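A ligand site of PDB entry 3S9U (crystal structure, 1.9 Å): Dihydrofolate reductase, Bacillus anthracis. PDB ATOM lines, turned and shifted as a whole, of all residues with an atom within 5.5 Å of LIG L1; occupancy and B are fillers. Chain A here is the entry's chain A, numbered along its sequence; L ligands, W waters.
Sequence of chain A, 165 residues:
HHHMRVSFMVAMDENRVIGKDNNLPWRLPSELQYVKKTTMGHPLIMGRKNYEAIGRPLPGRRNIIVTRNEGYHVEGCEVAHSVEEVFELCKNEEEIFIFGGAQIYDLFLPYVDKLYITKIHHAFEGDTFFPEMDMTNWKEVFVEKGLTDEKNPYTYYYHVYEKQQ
Water W1 lies within hydrogen-bond range of the side-chain amide oxygen of Asn 50, an oxygen (O1) of LIG L1 and an oxygen (O13) of LG2 L2.
Water W3 lies within hydrogen-bond range of OE1 of Glu 31 (2.7 Å) and NE1 of Trp 26 (2.8 Å).
OH of Tyr 105 is in hydrogen-bond range of O of Phe 99, 3.3 Å away.
The backbone NH (N) of Val 10 lies within hydrogen-bond range of the backbone carbonyl oxygen (O) of Tyr 116, 3.0 Å away.
The backbone carbonyl oxygen (O) of Gly 100 is in hydrogen-bond range of the side-chain amide nitrogen (ND2) of Asn 50, at 3.1 Å.
The side-chain hydroxyl (OH) of Tyr 105 lies close to the backbone NH (N) of Gly 100 (3.4 Å).
The backbone carbonyl oxygen (O) of Met 9 lies within hydrogen-bond range of the side-chain hydroxyl (OH) of Tyr 105.
O of Ile 54 sits at hydrogen-bond distance from NH1 of Arg 56, 3.3 Å away.
The backbone carbonyl oxygen (O) of Phe 99 lies within hydrogen-bond range of the side-chain amide nitrogen (ND2) of Asn 50 (3.1 Å).
OE2 of Glu 31 sits at hydrogen-bond distance from OG1 of Thr 118.
The backbone NH of Ala 11 lies close to a nitrogen (N3) of LIG L1, at 3.5 Å.
Merely in contact with LIG L1: Asn 23 (3.4 Å), Val 35 (3.4 Å), Asn 50 (3.5 Å), Ile 54 (3.6 Å), Leu 32 (3.6 Å), Lys 36 (3.7 Å), Leu 58 (3.7 Å), Tyr 105 (3.7 Å), Leu 24 (3.7 Å), Arg 56 (3.7 Å), Thr 118 (3.8 Å) and Ala 53 (3.95 Å).
Hydrophobic or aromatic side chains that line LIG L1: Met 9, Ala 11, Leu 24, Leu 32, Val 35, Ile 54, Leu 58 and Phe 99.
The nearest printed residue that does not touch LIG L1 is Arg 61 (4.5 Å).
O of Val 10 sits at hydrogen-bond distance from N3 of LIG L1, 3.3 Å away.
N3 of LIG L1 is in hydrogen-bond range of OE2 of Glu 31 (2.8 Å).
N of Asn 23 sits at hydrogen-bond distance from O12 of LG2 L2 (3.2 Å).
O of Ala 11 lies within hydrogen-bond range of N7 of LG2 L2 (2.8 Å).
The backbone NH (N) of Ala 11 is in hydrogen-bond range of an oxygen (O14) of LG2 L2 (2.8 Å).
N of Val 10 sits close to N1 of LIG L1 (3.4 Å).
The backbone carbonyl oxygen of Phe 99 sits at hydrogen-bond distance from a nitrogen (N4) of LIG L1, at 3.3 Å.
The backbone NH of Asn 50 is in hydrogen-bond range of an oxygen (O2) of LG2 L2 (3.0 Å).
O13 of LG2 L2 sits close to O of Asn 23, 3.3 Å away.
A nitrogen (N4) of LIG L1 lies within hydrogen-bond range of the backbone carbonyl oxygen of Met 9, at 3.1 Å.
SD of Met 9 is in hydrogen-bond range of N3 of LIG L1 (3.5 Å).
An oxygen (O14) of LG2 L2 lies close to a nitrogen (N4) of LIG L1.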
ATOM      1  N   MET A   9      11.037  25.259  31.332  1.00  0.00           N
ATOM      2  CA  MET A   9      12.335  25.367  31.986  1.00  0.00           C
ATOM      3  C   MET A   9      12.747  26.843  31.979  1.00  0.00           C
ATOM      4  O   MET A   9      12.948  27.416  30.910  1.00  0.00           O
ATOM      5  CB  MET A   9      13.368  24.501  31.253  1.00  0.00           C
ATOM      6  CG  MET A   9      14.813  24.675  31.739  1.00  0.00           C
ATOM      7  SD  MET A   9      15.087  24.250  33.474  1.00  0.00           S
ATOM      8  CE  MET A   9      14.855  22.471  33.434  1.00  0.00           C
ATOM      9  N   VAL A  10      12.854  27.433  33.171  1.00  0.00           N
ATOM     10  CA  VAL A  10      13.107  28.875  33.295  1.00  0.00           C
ATOM     11  C   VAL A  10      13.876  29.230  34.570  1.00  0.00           C
ATOM     12  O   VAL A  10      13.741  28.564  35.598  1.00  0.00           O
ATOM     13  CB  VAL A  10      11.784  29.701  33.204  1.00  0.00           C
ATOM     14  CG1 VAL A  10      10.875  29.435  34.394  1.00  0.00           C
ATOM     15  CG2 VAL A  10      12.061  31.203  33.060  1.00  0.00           C
ATOM     16  N   ALA A  11      14.713  30.270  34.484  1.00  0.00           N
ATOM     17  CA  ALA A  11      15.338  30.885  35.658  1.00  0.00           C
ATOM     18  C   ALA A  11      14.941  32.360  35.708  1.00  0.00           C
ATOM     19  O   ALA A  11      15.096  33.076  34.715  1.00  0.00           O
ATOM     20  CB  ALA A  11      16.847  30.731  35.608  1.00  0.00           C
ATOM     21  N   ASN A  23      19.995  39.138  26.468  1.00  0.00           N
ATOM     22  CA  ASN A  23      20.935  38.210  27.102  1.00  0.00           C
ATOM     23  C   ASN A  23      20.474  37.895  28.531  1.00  0.00           C
ATOM     24  O   ASN A  23      19.469  38.457  28.997  1.00  0.00           O
ATOM     25  CB  ASN A  23      22.335  38.819  27.119  1.00  0.00           C
ATOM     26  CG  ASN A  23      23.447  37.765  27.060  1.00  0.00           C
ATOM     27  OD1 ASN A  23      23.245  36.594  27.408  1.00  0.00           O
ATOM     28  ND2 ASN A  23      24.630  38.191  26.617  1.00  0.00           N
ATOM     29  N   LEU A  24      21.173  36.997  29.208  1.00  0.00           N
ATOM     30  CA  LEU A  24      20.904  36.697  30.614  1.00  0.00           C
ATOM     31  C   LEU A  24      21.533  37.762  31.505  1.00  0.00           C
ATOM     32  O   LEU A  24      22.651  38.202  31.237  1.00  0.00           O
ATOM     33  CB  LEU A  24      21.432  35.315  30.995  1.00  0.00           C
ATOM     34  CG  LEU A  24      20.903  34.088  30.235  1.00  0.00           C
ATOM     35  CD1 LEU A  24      21.729  32.860  30.570  1.00  0.00           C
ATOM     36  CD2 LEU A  24      19.433  33.839  30.558  1.00  0.00           C
ATOM     37  N   TRP A  26      22.518  37.376  34.597  1.00  0.00           N
ATOM     38  CA  TRP A  26      23.431  36.739  35.557  1.00  0.00           C
ATOM     39  C   TRP A  26      24.237  35.629  34.901  1.00  0.00           C
ATOM     40  O   TRP A  26      23.883  35.156  33.812  1.00  0.00           O
ATOM     41  CB  TRP A  26      22.630  36.136  36.726  1.00  0.00           C
ATOM     42  CG  TRP A  26      21.548  35.218  36.250  1.00  0.00           C
ATOM     43  CD1 TRP A  26      21.688  33.902  35.877  1.00  0.00           C
ATOM     44  CD2 TRP A  26      20.174  35.544  36.055  1.00  0.00           C
ATOM     45  NE1 TRP A  26      20.473  33.395  35.484  1.00  0.00           N
ATOM     46  CE2 TRP A  26      19.522  34.384  35.568  1.00  0.00           C
ATOM     47  CE3 TRP A  26      19.418  36.704  36.245  1.00  0.00           C
ATOM     48  CZ2 TRP A  26      18.163  34.353  35.280  1.00  0.00           C
ATOM     49  CZ3 TRP A  26      18.058  36.674  35.958  1.00  0.00           C
ATOM     50  CH2 TRP A  26      17.447  35.510  35.479  1.00  0.00           C
ATOM     51  N   GLU A  31      23.868  26.471  37.789  1.00  0.00           N
ATOM     52  CA  GLU A  31      22.480  26.474  37.352  1.00  0.00           C
ATOM     53  C   GLU A  31      22.372  25.923  35.929  1.00  0.00           C
ATOM     54  O   GLU A  31      21.475  25.154  35.623  1.00  0.00           O
ATOM     55  CB  GLU A  31      21.908  27.895  37.441  1.00  0.00           C
ATOM     56  CG  GLU A  31      20.388  27.969  37.681  1.00  0.00           C
ATOM     57  CD  GLU A  31      19.577  27.801  36.412  1.00  0.00           C
ATOM     58  OE1 GLU A  31      20.024  28.257  35.341  1.00  0.00           O
ATOM     59  OE2 GLU A  31      18.471  27.207  36.482  1.00  0.00           O
ATOM     60  N   LEU A  32      23.318  26.314  35.079  1.00  0.00           N
ATOM     61  CA  LEU A  32      23.386  25.812  33.711  1.00  0.00           C
ATOM     62  C   LEU A  32      23.574  24.288  33.708  1.00  0.00           C
ATOM     63  O   LEU A  32      22.997  23.597  32.880  1.00  0.00           O
ATOM     64  CB  LEU A  32      24.507  26.509  32.933  1.00  0.00           C
ATOM     65  CG  LEU A  32      24.848  26.058  31.517  1.00  0.00           C
ATOM     66  CD1 LEU A  32      23.690  26.306  30.561  1.00  0.00           C
ATOM     67  CD2 LEU A  32      26.091  26.778  31.013  1.00  0.00           C
ATOM     68  N   TYR A  34      22.507  22.216  36.010  1.00  0.00           N
ATOM     69  CA  TYR A  34      21.200  21.667  36.348  1.00  0.00           C
ATOM     70  C   TYR A  34      20.280  21.624  35.127  1.00  0.00           C
ATOM     71  O   TYR A  34      19.554  20.646  34.928  1.00  0.00           O
ATOM     72  CB  TYR A  34      20.566  22.495  37.478  1.00  0.00           C
ATOM     73  CG  TYR A  34      19.113  22.176  37.759  1.00  0.00           C
ATOM     74  CD1 TYR A  34      18.087  22.898  37.148  1.00  0.00           C
ATOM     75  CD2 TYR A  34      18.769  21.159  38.640  1.00  0.00           C
ATOM     76  CE1 TYR A  34      16.753  22.620  37.420  1.00  0.00           C
ATOM     77  CE2 TYR A  34      17.429  20.864  38.910  1.00  0.00           C
ATOM     78  CZ  TYR A  34      16.430  21.600  38.299  1.00  0.00           C
ATOM     79  OH  TYR A  34      15.109  21.318  38.566  1.00  0.00           O
ATOM     80  N   VAL A  35      20.303  22.688  34.338  1.00  0.00           N
ATOM     81  CA  VAL A  35      19.514  22.761  33.099  1.00  0.00           C
ATOM     82  C   VAL A  35      19.906  21.628  32.143  1.00  0.00           C
ATOM     83  O   VAL A  35      19.027  20.926  31.634  1.00  0.00           O
ATOM     84  CB  VAL A  35      19.697  24.133  32.401  1.00  0.00           C
ATOM     85  CG1 VAL A  35      19.087  24.120  30.994  1.00  0.00           C
ATOM     86  CG2 VAL A  35      19.070  25.244  33.247  1.00  0.00           C
ATOM     87  N   LYS A  36      21.211  21.474  31.919  1.00  0.00           N
ATOM     88  CA  LYS A  36      21.727  20.435  31.008  1.00  0.00           C
ATOM     89  C   LYS A  36      21.307  19.045  31.459  1.00  0.00           C
ATOM     90  O   LYS A  36      20.804  18.257  30.658  1.00  0.00           O
ATOM     91  CB  LYS A  36      23.257  20.528  30.893  1.00  0.00           C
ATOM     92  CG  LYS A  36      23.763  21.715  30.076  1.00  0.00           C
ATOM     93  CD  LYS A  36      25.285  21.816  30.127  1.00  0.00           C
ATOM     94  CE  LYS A  36      25.788  23.003  29.323  1.00  0.00           C
ATOM     95  NZ  LYS A  36      27.273  23.152  29.382  1.00  0.00           N
ATOM     96  N   LEU A  44      14.052  20.795  23.039  1.00  0.00           N
ATOM     97  CA  LEU A  44      14.012  22.171  23.552  1.00  0.00           C
ATOM     98  C   LEU A  44      13.276  23.039  22.561  1.00  0.00           C
ATOM     99  O   LEU A  44      13.622  23.070  21.378  1.00  0.00           O
ATOM    100  CB  LEU A  44      15.429  22.729  23.744  1.00  0.00           C
ATOM    101  CG  LEU A  44      16.348  22.139  24.808  1.00  0.00           C
ATOM    102  CD1 LEU A  44      17.660  22.892  24.805  1.00  0.00           C
ATOM    103  CD2 LEU A  44      15.710  22.185  26.200  1.00  0.00           C
ATOM    104  N   ASN A  50      15.630  33.913  21.609  1.00  0.00           N
ATOM    105  CA  ASN A  50      16.366  33.028  22.527  1.00  0.00           C
ATOM    106  C   ASN A  50      17.379  32.185  21.761  1.00  0.00           C
ATOM    107  O   ASN A  50      18.559  32.154  22.123  1.00  0.00           O
ATOM    108  CB  ASN A  50      15.395  32.131  23.307  1.00  0.00           C
ATOM    109  CG  ASN A  50      16.092  31.231  24.324  1.00  0.00           C
ATOM    110  OD1 ASN A  50      17.206  31.520  24.772  1.00  0.00           O
ATOM    111  ND2 ASN A  50      15.441  30.136  24.687  1.00  0.00           N
ATOM    112  N   ALA A  53      20.409  34.150  20.530  1.00  0.00           N
ATOM    113  CA  ALA A  53      21.246  34.528  21.668  1.00  0.00           C
ATOM    114  C   ALA A  53      22.094  33.352  22.170  1.00  0.00           C
ATOM    115  O   ALA A  53      23.246  33.534  22.579  1.00  0.00           O
ATOM    116  CB  ALA A  53      20.406  35.102  22.793  1.00  0.00           C
ATOM    117  N   ILE A  54      21.518  32.147  22.146  1.00  0.00           N
ATOM    118  CA  ILE A  54      22.264  30.926  22.450  1.00  0.00           C
ATOM    119  C   ILE A  54      23.349  30.721  21.387  1.00  0.00           C
ATOM    120  O   ILE A  54      24.517  30.495  21.709  1.00  0.00           O
ATOM    121  CB  ILE A  54      21.332  29.685  22.594  1.00  0.00           C
ATOM    122  CG1 ILE A  54      20.382  29.870  23.787  1.00  0.00           C
ATOM    123  CG2 ILE A  54      22.139  28.397  22.757  1.00  0.00           C
ATOM    124  CD1 ILE A  54      19.183  28.921  23.814  1.00  0.00           C
ATOM    125  N   ARG A  56      23.938  28.517  18.864  1.00  0.00           N
ATOM    126  CA  ARG A  56      24.316  27.212  18.318  1.00  0.00           C
ATOM    127  C   ARG A  56      23.271  26.156  18.684  1.00  0.00           C
ATOM    128  O   ARG A  56      22.568  26.295  19.690  1.00  0.00           O
ATOM    129  CB  ARG A  56      25.709  26.808  18.847  1.00  0.00           C
ATOM    130  CG  ARG A  56      25.731  26.464  20.336  1.00  0.00           C
ATOM    131  CD  ARG A  56      27.091  26.669  20.972  1.00  0.00           C
ATOM    132  NE  ARG A  56      27.123  26.187  22.348  1.00  0.00           N
ATOM    133  CZ  ARG A  56      26.712  26.876  23.411  1.00  0.00           C
ATOM    134  NH1 ARG A  56      26.221  28.104  23.285  1.00  0.00           N
ATOM    135  NH2 ARG A  56      26.780  26.328  24.619  1.00  0.00           N
ATOM    136  N   LEU A  58      22.083  22.943  20.477  1.00  0.00           N
ATOM    137  CA  LEU A  58      22.537  22.236  21.674  1.00  0.00           C
ATOM    138  C   LEU A  58      22.544  20.731  21.415  1.00  0.00           C
ATOM    139  O   LEU A  58      21.533  20.163  20.992  1.00  0.00           O
ATOM    140  CB  LEU A  58      21.663  22.589  22.890  1.00  0.00           C
ATOM    141  CG  LEU A  58      21.688  24.013  23.478  1.00  0.00           C
ATOM    142  CD1 LEU A  58      23.055  24.691  23.324  1.00  0.00           C
ATOM    143  CD2 LEU A  58      20.592  24.892  22.888  1.00  0.00           C
ATOM    144  N   ARG A  61      19.962  16.808  21.747  1.00  0.00           N
ATOM    145  CA  ARG A  61      18.566  17.243  21.892  1.00  0.00           C
ATOM    146  C   ARG A  61      17.989  17.672  20.547  1.00  0.00           C
ATOM    147  O   ARG A  61      18.725  18.152  19.670  1.00  0.00           O
ATOM    148  CB  ARG A  61      18.477  18.407  22.878  1.00  0.00           C
ATOM    149  CG  ARG A  61      18.563  18.029  24.357  1.00  0.00           C
ATOM    150  CD  ARG A  61      18.739  19.249  25.230  1.00  0.00           C
ATOM    151  NE  ARG A  61      20.078  19.824  25.044  1.00  0.00           N
ATOM    152  CZ  ARG A  61      21.052  19.781  25.947  1.00  0.00           C
ATOM    153  NH1 ARG A  61      20.851  19.225  27.132  1.00  0.00           N
ATOM    154  NH2 ARG A  61      22.230  20.325  25.667  1.00  0.00           N
ATOM    155  N   PHE A  99      11.690  26.503  26.487  1.00  0.00           N
ATOM    156  CA  PHE A  99      12.993  26.976  26.955  1.00  0.00           C
ATOM    157  C   PHE A  99      13.109  28.502  26.930  1.00  0.00           C
ATOM    158  O   PHE A  99      14.157  29.057  27.252  1.00  0.00           O
ATOM    159  CB  PHE A  99      14.088  26.344  26.086  1.00  0.00           C
ATOM    160  CG  PHE A  99      15.439  26.247  26.757  1.00  0.00           C
ATOM    161  CD1 PHE A  99      15.606  25.497  27.912  1.00  0.00           C
ATOM    162  CD2 PHE A  99      16.543  26.891  26.212  1.00  0.00           C
ATOM    163  CE1 PHE A  99      16.855  25.393  28.525  1.00  0.00           C
ATOM    164  CE2 PHE A  99      17.804  26.790  26.813  1.00  0.00           C
ATOM    165  CZ  PHE A  99      17.958  26.044  27.973  1.00  0.00           C
ATOM    166  N   GLY A 100      12.016  29.188  26.557  1.00  0.00           N
ATOM    167  CA  GLY A 100      12.010  30.658  26.481  1.00  0.00           C
ATOM    168  C   GLY A 100      12.228  31.209  25.089  1.00  0.00           C
ATOM    169  O   GLY A 100      12.450  30.448  24.149  1.00  0.00           O
ATOM    170  N   TYR A 105       7.148  31.601  26.210  1.00  0.00           N
ATOM    171  CA  TYR A 105       6.463  31.214  27.450  1.00  0.00           C
ATOM    172  C   TYR A 105       4.987  31.618  27.424  1.00  0.00           C
ATOM    173  O   TYR A 105       4.122  30.824  27.804  1.00  0.00           O
ATOM    174  CB  TYR A 105       7.130  31.812  28.691  1.00  0.00           C
ATOM    175  CG  TYR A 105       8.505  31.261  29.015  1.00  0.00           C
ATOM    176  CD1 TYR A 105       8.751  29.884  29.045  1.00  0.00           C
ATOM    177  CD2 TYR A 105       9.559  32.118  29.316  1.00  0.00           C
ATOM    178  CE1 TYR A 105      10.018  29.385  29.356  1.00  0.00           C
ATOM    179  CE2 TYR A 105      10.823  31.639  29.619  1.00  0.00           C
ATOM    180  CZ  TYR A 105      11.046  30.271  29.644  1.00  0.00           C
ATOM    181  OH  TYR A 105      12.309  29.806  29.933  1.00  0.00           O
ATOM    182  N   TYR A 116       9.613  23.785  35.784  1.00  0.00           N
ATOM    183  CA  TYR A 116      10.945  23.732  36.388  1.00  0.00           C
ATOM    184  C   TYR A 116      11.435  25.164  36.461  1.00  0.00           C
ATOM    185  O   TYR A 116      11.905  25.716  35.456  1.00  0.00           O
ATOM    186  CB  TYR A 116      11.915  22.906  35.555  1.00  0.00           C
ATOM    187  CG  TYR A 116      11.541  21.459  35.362  1.00  0.00           C
ATOM    188  CD1 TYR A 116      10.529  21.089  34.469  1.00  0.00           C
ATOM    189  CD2 TYR A 116      12.225  20.455  36.046  1.00  0.00           C
ATOM    190  CE1 TYR A 116      10.202  19.743  34.275  1.00  0.00           C
ATOM    191  CE2 TYR A 116      11.898  19.109  35.852  1.00  0.00           C
ATOM    192  CZ  TYR A 116      10.889  18.761  34.968  1.00  0.00           C
ATOM    193  OH  TYR A 116      10.566  17.439  34.769  1.00  0.00           O
ATOM    194  N   THR A 118      13.820  28.030  38.416  1.00  0.00           N
ATOM    195  CA  THR A 118      14.868  28.441  39.333  1.00  0.00           C
ATOM    196  C   THR A 118      14.578  29.871  39.759  1.00  0.00           C
ATOM    197  O   THR A 118      14.369  30.746  38.918  1.00  0.00           O
ATOM    198  CB  THR A 118      16.264  28.349  38.682  1.00  0.00           C
ATOM    199  OG1 THR A 118      16.483  27.016  38.216  1.00  0.00           O
ATOM    200  CG2 THR A 118      17.356  28.714  39.694  1.00  0.00           C
HETATM  201  N1  LIG L   1      16.122  27.826  32.243  1.00  0.00           N
HETATM  202  C1  LIG L   1      16.911  27.875  33.335  1.00  0.00           C
HETATM  203  N2  LIG L   1      18.107  28.501  33.294  1.00  0.00           N
HETATM  204  C2  LIG L   1      18.545  29.101  32.184  1.00  0.00           C
HETATM  205  C3  LIG L   1      17.745  29.055  31.039  1.00  0.00           C
HETATM  206  C4  LIG L   1      16.513  28.397  31.092  1.00  0.00           C
HETATM  207  C5  LIG L   1      21.029  28.791  31.910  1.00  0.00           C
HETATM  208  C6  LIG L   1      22.389  33.457  26.437  1.00  0.00           C
HETATM  209  N3  LIG L   1      16.517  27.295  34.463  1.00  0.00           N
HETATM  210  N4  LIG L   1      15.721  28.340  30.021  1.00  0.00           N
HETATM  211  C7  LIG L   1      18.622  30.226  28.845  1.00  0.00           C
HETATM  212  C8  LIG L   1      18.212  29.691  29.849  1.00  0.00           C
HETATM  213  C9  LIG L   1      23.025  24.395  27.360  1.00  0.00           C
HETATM  214  C10 LIG L   1      21.785  24.878  27.786  1.00  0.00           C
HETATM  215  C11 LIG L   1      23.974  25.291  26.864  1.00  0.00           C
HETATM  216  C12 LIG L   1      21.502  26.236  27.711  1.00  0.00           C
HETATM  217  C13 LIG L   1      23.677  26.653  26.794  1.00  0.00           C
HETATM  218  C14 LIG L   1      23.147  29.418  26.747  1.00  0.00           C
HETATM  219  C15 LIG L   1      22.876  30.786  26.653  1.00  0.00           C
HETATM  220  C16 LIG L   1      20.873  29.028  27.412  1.00  0.00           C
HETATM  221  C17 LIG L   1      19.923  29.785  32.250  1.00  0.00           C
HETATM  222  C18 LIG L   1      19.148  30.886  27.648  1.00  0.00           C
HETATM  223  O1  LIG L   1      21.298  32.609  26.846  1.00  0.00           O
HETATM  224  C19 LIG L   1      22.434  27.149  27.220  1.00  0.00           C
HETATM  225  C20 LIG L   1      22.150  28.522  27.130  1.00  0.00           C
HETATM  226  C21 LIG L   1      20.579  30.398  27.320  1.00  0.00           C
HETATM  227  C22 LIG L   1      21.593  31.277  26.933  1.00  0.00           C
HETATM  228  P1  LG2 L   2      11.689  34.917  22.351  1.00  0.00           P
HETATM  229  O1  LG2 L   2      10.407  34.541  22.978  1.00  0.00           O
HETATM  230  O2  LG2 L   2      12.802  34.009  22.668  1.00  0.00           O
HETATM  231  O3  LG2 L   2      11.508  35.033  20.767  1.00  0.00           O
HETATM  232  C1  LG2 L   2      10.570  35.927  20.212  1.00  0.00           C
HETATM  233  C2  LG2 L   2      10.372  35.476  18.782  1.00  0.00           C
HETATM  234  O4  LG2 L   2       9.610  34.286  18.769  1.00  0.00           O
HETATM  235  C3  LG2 L   2       9.594  36.460  17.925  1.00  0.00           C
HETATM  236  O5  LG2 L   2      10.410  37.510  17.451  1.00  0.00           O
HETATM  237  C4  LG2 L   2       9.126  35.523  16.828  1.00  0.00           C
HETATM  238  O6  LG2 L   2      10.169  35.221  15.925  1.00  0.00           O
HETATM  239  C5  LG2 L   2       8.816  34.241  17.596  1.00  0.00           C
HETATM  240  N1  LG2 L   2       7.384  34.223  17.938  1.00  0.00           N
HETATM  241  C6  LG2 L   2       6.769  34.929  18.943  1.00  0.00           C
HETATM  242  N2  LG2 L   2       5.451  34.643  18.922  1.00  0.00           N
HETATM  243  C7  LG2 L   2       5.221  33.779  17.901  1.00  0.00           C
HETATM  244  C8  LG2 L   2       4.059  33.170  17.443  1.00  0.00           C
HETATM  245  N3  LG2 L   2       2.901  33.420  18.029  1.00  0.00           N
HETATM  246  N4  LG2 L   2       4.129  32.306  16.364  1.00  0.00           N
HETATM  247  C9  LG2 L   2       5.348  32.050  15.755  1.00  0.00           C
HETATM  248  N5  LG2 L   2       6.497  32.656  16.224  1.00  0.00           N
HETATM  249  C10 LG2 L   2       6.424  33.504  17.287  1.00  0.00           C
HETATM  250  O7  LG2 L   2      12.065  36.448  22.715  1.00  0.00           O
HETATM  251  P2  LG2 L   2      11.911  37.350  24.023  1.00  0.00           P
HETATM  252  O8  LG2 L   2      12.477  38.672  23.666  1.00  0.00           O
HETATM  253  O9  LG2 L   2      10.537  37.263  24.563  1.00  0.00           O
HETATM  254  O10 LG2 L   2      12.892  36.623  25.073  1.00  0.00           O
HETATM  255  C11 LG2 L   2      14.297  36.665  24.871  1.00  0.00           C
HETATM  256  C12 LG2 L   2      14.978  37.092  26.166  1.00  0.00           C
HETATM  257  O11 LG2 L   2      14.702  36.161  27.203  1.00  0.00           O
HETATM  258  C13 LG2 L   2      16.487  37.134  26.016  1.00  0.00           C
HETATM  259  O12 LG2 L   2      16.955  38.234  26.779  1.00  0.00           O
HETATM  260  C14 LG2 L   2      16.959  35.836  26.641  1.00  0.00           C
HETATM  261  O13 LG2 L   2      18.261  35.943  27.181  1.00  0.00           O
HETATM  262  C15 LG2 L   2      15.916  35.635  27.733  1.00  0.00           C
HETATM  263  N6  LG2 L   2      15.717  34.239  28.151  1.00  0.00           N
HETATM  264  C16 LG2 L   2      15.887  33.955  29.479  1.00  0.00           C
HETATM  265  C17 LG2 L   2      15.710  32.661  29.957  1.00  0.00           C
HETATM  266  C18 LG2 L   2      15.820  32.392  31.432  1.00  0.00           C
HETATM  267  O14 LG2 L   2      15.314  31.199  31.931  1.00  0.00           O
HETATM  268  N7  LG2 L   2      16.398  33.295  32.233  1.00  0.00           N
HETATM  269  C19 LG2 L   2      15.320  31.653  29.070  1.00  0.00           C
HETATM  270  C20 LG2 L   2      15.137  31.963  27.726  1.00  0.00           C
HETATM  271  C21 LG2 L   2      15.338  33.264  27.267  1.00  0.00           C
HETATM  272  P3  LG2 L   2      10.368  35.993  14.531  1.00  0.00           P
HETATM  273  O15 LG2 L   2       9.075  35.899  13.748  1.00  0.00           O
HETATM  274  O16 LG2 L   2      10.693  37.443  14.844  1.00  0.00           O
HETATM  275  O17 LG2 L   2      11.515  35.378  13.789  1.00  0.00           O
HETATM  276  O   HOH W   1      18.952  33.449  25.355  1.00  0.00           O
HETATM  277  O   HOH W   2      14.640  25.522  36.741  1.00  0.00           O
HETATM  278  O   HOH W   3      21.224  30.707  35.169  1.00  0.00           O
